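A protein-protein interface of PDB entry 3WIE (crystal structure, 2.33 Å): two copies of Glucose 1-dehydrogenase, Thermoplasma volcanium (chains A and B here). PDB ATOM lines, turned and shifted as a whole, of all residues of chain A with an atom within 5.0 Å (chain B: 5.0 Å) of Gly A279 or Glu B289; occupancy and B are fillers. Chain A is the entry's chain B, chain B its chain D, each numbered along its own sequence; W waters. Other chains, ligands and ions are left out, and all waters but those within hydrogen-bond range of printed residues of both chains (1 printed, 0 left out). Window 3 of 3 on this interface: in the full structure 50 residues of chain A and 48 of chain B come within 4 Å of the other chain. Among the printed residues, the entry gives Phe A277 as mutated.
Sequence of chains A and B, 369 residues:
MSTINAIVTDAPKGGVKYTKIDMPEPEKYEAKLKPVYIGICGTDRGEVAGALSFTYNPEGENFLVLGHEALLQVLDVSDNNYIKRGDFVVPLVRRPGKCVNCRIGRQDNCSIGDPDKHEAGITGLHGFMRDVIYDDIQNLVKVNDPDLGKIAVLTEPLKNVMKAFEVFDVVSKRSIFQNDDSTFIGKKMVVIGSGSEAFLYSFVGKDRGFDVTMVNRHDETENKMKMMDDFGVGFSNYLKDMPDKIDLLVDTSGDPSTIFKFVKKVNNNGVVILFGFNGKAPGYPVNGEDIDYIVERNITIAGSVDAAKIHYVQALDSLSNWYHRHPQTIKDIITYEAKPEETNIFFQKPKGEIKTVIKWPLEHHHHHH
The backbone NH of Gly B288 lies within hydrogen-bond range of the backbone carbonyl oxygen of Ala A281 (3.1 Å).
N of Lys A280 lies close to OD1 of Asn A278. The side-chain amide oxygen (OD1) of Asn B287 sits at hydrogen-bond distance from the backbone NH (N) of Glu B289, at 3.1 Å. The backbone NH (N) of Asn B287 lies within hydrogen-bond range of the side-chain carboxylate (OD2) of Asp B290 (2.8 Å).
CG of Phe A277 touches OD1 of Asp B292, 3.7 Å away. Gly B288 touches Asn A278 (CA to O, 3.0 Å). Gly A279 touches Glu B289. O of Ala A281 touches CB of Asn B287 (3.8 Å).
Of the printed residues of chain B, Phe A277 touches Asp B292 (3.7 Å). Of the printed residues of chain B, Asn A278 touches Gly B288 (3.0 Å). Gly A279 touches just one residue of chain B: Glu B289. Of chain A, only Gly A279 comes within 4 Å of Glu B289. Of the printed residues of chain A, Asp B292 touches Phe A277. The nearest residue of chain A that does not touch Glu B289 is Asn A278 (4.2 Å). The nearest printed residue of chain A that does not touch Asn B287 is Gly A279 (5.2 Å).
Hydrophobic or aromatic side chains of chain A that line the printed part of chain B: Phe A277. Among the printed residues, 5 pairs touch across the chains.
No position is printed for both chains.
Water W1 bridges the backbone carbonyl oxygen of Gly B288 (2.6 Å) and the backbone NH of Asn A278 (2.9 Å).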
ATOM      1  N   PHE A 277       6.779  24.407 -15.111  1.00  0.00           N
ATOM      2  CA  PHE A 277       6.582  24.294 -13.675  1.00  0.00           C
ATOM      3  C   PHE A 277       5.406  25.113 -13.168  1.00  0.00           C
ATOM      4  O   PHE A 277       5.215  26.258 -13.545  1.00  0.00           O
ATOM      5  CB  PHE A 277       7.854  24.565 -12.855  1.00  0.00           C
ATOM      6  CG  PHE A 277       8.516  25.890 -13.127  1.00  0.00           C
ATOM      7  CD1 PHE A 277       8.019  27.070 -12.564  1.00  0.00           C
ATOM      8  CD2 PHE A 277       9.679  25.954 -13.916  1.00  0.00           C
ATOM      9  CE1 PHE A 277       8.648  28.289 -12.813  1.00  0.00           C
ATOM     10  CE2 PHE A 277      10.307  27.166 -14.160  1.00  0.00           C
ATOM     11  CZ  PHE A 277       9.790  28.335 -13.614  1.00  0.00           C
ATOM     12  N   ASN A 278       4.620  24.458 -12.331  1.00  0.00           N
ATOM     13  CA  ASN A 278       3.462  25.012 -11.701  1.00  0.00           C
ATOM     14  C   ASN A 278       3.398  24.407 -10.307  1.00  0.00           C
ATOM     15  O   ASN A 278       2.996  23.248 -10.132  1.00  0.00           O
ATOM     16  CB  ASN A 278       2.223  24.634 -12.471  1.00  0.00           C
ATOM     17  CG  ASN A 278       0.957  25.250 -11.871  1.00  0.00           C
ATOM     18  OD1 ASN A 278       0.996  26.104 -10.966  1.00  0.00           O
ATOM     19  ND2 ASN A 278      -0.162  24.818 -12.367  1.00  0.00           N
ATOM     20  N   GLY A 279       3.868  25.166  -9.328  1.00  0.00           N
ATOM     21  CA  GLY A 279       3.830  24.748  -7.925  1.00  0.00           C
ATOM     22  C   GLY A 279       2.428  24.425  -7.377  1.00  0.00           C
ATOM     23  O   GLY A 279       2.318  23.606  -6.444  1.00  0.00           O
ATOM     24  N   LYS A 280       1.388  25.040  -7.960  1.00  0.00           N
ATOM     25  CA  LYS A 280      -0.021  24.801  -7.560  1.00  0.00           C
ATOM     26  C   LYS A 280      -0.657  23.520  -8.098  1.00  0.00           C
ATOM     27  O   LYS A 280      -1.705  23.129  -7.612  1.00  0.00           O
ATOM     28  CB  LYS A 280      -0.926  26.001  -7.931  1.00  0.00           C
ATOM     29  CG  LYS A 280      -0.725  27.224  -7.023  1.00  0.00           C
ATOM     30  CD  LYS A 280      -1.518  28.465  -7.460  1.00  0.00           C
ATOM     31  CE  LYS A 280      -1.056  29.035  -8.812  1.00  0.00           C
ATOM     32  NZ  LYS A 280      -1.271  30.510  -8.985  1.00  0.00           N
ATOM     33  N   ALA A 281      -0.042  22.851  -9.076  1.00  0.00           N
ATOM     34  CA  ALA A 281      -0.697  21.705  -9.734  1.00  0.00           C
ATOM     35  C   ALA A 281      -0.828  20.552  -8.773  1.00  0.00           C
ATOM     36  O   ALA A 281       0.037  20.354  -7.936  1.00  0.00           O
ATOM     37  CB  ALA A 281       0.061  21.267 -10.983  1.00  0.00           C
ATOM     38  N   ASN B 287       3.317  15.993  -6.873  1.00  0.00           N
ATOM     39  CA  ASN B 287       2.663  17.262  -7.215  1.00  0.00           C
ATOM     40  C   ASN B 287       3.539  18.296  -7.990  1.00  0.00           C
ATOM     41  O   ASN B 287       4.729  18.135  -8.178  1.00  0.00           O
ATOM     42  CB  ASN B 287       2.094  17.887  -5.958  1.00  0.00           C
ATOM     43  CG  ASN B 287       3.153  18.542  -5.061  1.00  0.00           C
ATOM     44  OD1 ASN B 287       4.346  18.609  -5.369  1.00  0.00           O
ATOM     45  ND2 ASN B 287       2.687  19.063  -3.928  1.00  0.00           N
ATOM     46  N   GLY B 288       2.898  19.375  -8.383  1.00  0.00           N
ATOM     47  CA  GLY B 288       3.508  20.503  -9.035  1.00  0.00           C
ATOM     48  C   GLY B 288       4.875  20.911  -8.544  1.00  0.00           C
ATOM     49  O   GLY B 288       5.772  21.186  -9.369  1.00  0.00           O
ATOM     50  N   GLU B 289       5.027  20.954  -7.223  1.00  0.00           N
ATOM     51  CA  GLU B 289       6.272  21.392  -6.576  1.00  0.00           C
ATOM     52  C   GLU B 289       7.356  20.342  -6.659  1.00  0.00           C
ATOM     53  O   GLU B 289       8.516  20.677  -6.746  1.00  0.00           O
ATOM     54  CB  GLU B 289       6.058  21.741  -5.095  1.00  0.00           C
ATOM     55  CG  GLU B 289       5.420  23.118  -4.891  1.00  0.00           C
ATOM     56  CD  GLU B 289       5.068  23.415  -3.428  1.00  0.00           C
ATOM     57  OE1 GLU B 289       5.781  22.917  -2.511  1.00  0.00           O
ATOM     58  OE2 GLU B 289       4.078  24.148  -3.199  1.00  0.00           O
ATOM     59  N   ASP B 290       6.983  19.074  -6.587  1.00  0.00           N
ATOM     60  CA  ASP B 290       7.935  18.013  -6.770  1.00  0.00           C
ATOM     61  C   ASP B 290       8.613  18.183  -8.173  1.00  0.00           C
ATOM     62  O   ASP B 290       9.831  18.234  -8.288  1.00  0.00           O
ATOM     63  CB  ASP B 290       7.244  16.673  -6.604  1.00  0.00           C
ATOM     64  CG  ASP B 290       6.526  16.546  -5.237  1.00  0.00           C
ATOM     65  OD1 ASP B 290       7.019  17.151  -4.256  1.00  0.00           O
ATOM     66  OD2 ASP B 290       5.465  15.870  -5.148  1.00  0.00           O
ATOM     67  N   ILE B 291       7.810  18.387  -9.199  1.00  0.00           N
ATOM     68  CA  ILE B 291       8.320  18.591 -10.555  1.00  0.00           C
ATOM     69  C   ILE B 291       9.299  19.789 -10.576  1.00  0.00           C
ATOM     70  O   ILE B 291      10.448  19.702 -11.026  1.00  0.00           O
ATOM     71  CB  ILE B 291       7.122  18.793 -11.534  1.00  0.00           C
ATOM     72  CG1 ILE B 291       6.213  17.577 -11.491  1.00  0.00           C
ATOM     73  CG2 ILE B 291       7.549  19.072 -12.972  1.00  0.00           C
ATOM     74  CD1 ILE B 291       6.965  16.286 -11.491  1.00  0.00           C
ATOM     75  N   ASP B 292       8.830  20.882 -10.038  1.00  0.00           N
ATOM     76  CA  ASP B 292       9.568  22.107  -9.987  1.00  0.00           C
ATOM     77  C   ASP B 292      10.901  21.915  -9.282  1.00  0.00           C
ATOM     78  O   ASP B 292      11.891  22.471  -9.699  1.00  0.00           O
ATOM     79  CB  ASP B 292       8.681  23.142  -9.262  1.00  0.00           C
ATOM     80  CG  ASP B 292       9.405  24.402  -8.902  1.00  0.00           C
ATOM     81  OD1 ASP B 292       9.944  25.034  -9.824  1.00  0.00           O
ATOM     82  OD2 ASP B 292       9.400  24.770  -7.696  1.00  0.00           O
ATOM     83  N   TYR B 293      10.922  21.127  -8.211  1.00  0.00           N
ATOM     84  CA  TYR B 293      12.160  20.784  -7.514  1.00  0.00           C
ATOM     85  C   TYR B 293      13.201  20.215  -8.517  1.00  0.00           C
ATOM     86  O   TYR B 293      14.354  20.608  -8.517  1.00  0.00           O
ATOM     87  CB  TYR B 293      11.887  19.735  -6.415  1.00  0.00           C
ATOM     88  CG  TYR B 293      13.103  19.479  -5.552  1.00  0.00           C
ATOM     89  CD1 TYR B 293      14.022  18.501  -5.896  1.00  0.00           C
ATOM     90  CD2 TYR B 293      13.344  20.231  -4.376  1.00  0.00           C
ATOM     91  CE1 TYR B 293      15.165  18.280  -5.143  1.00  0.00           C
ATOM     92  CE2 TYR B 293      14.484  20.008  -3.607  1.00  0.00           C
ATOM     93  CZ  TYR B 293      15.391  19.041  -3.992  1.00  0.00           C
ATOM     94  OH  TYR B 293      16.537  18.798  -3.257  1.00  0.00           O
HETATM   95  O   HOH W   1       5.209  21.619 -11.856  1.00  0.00           O
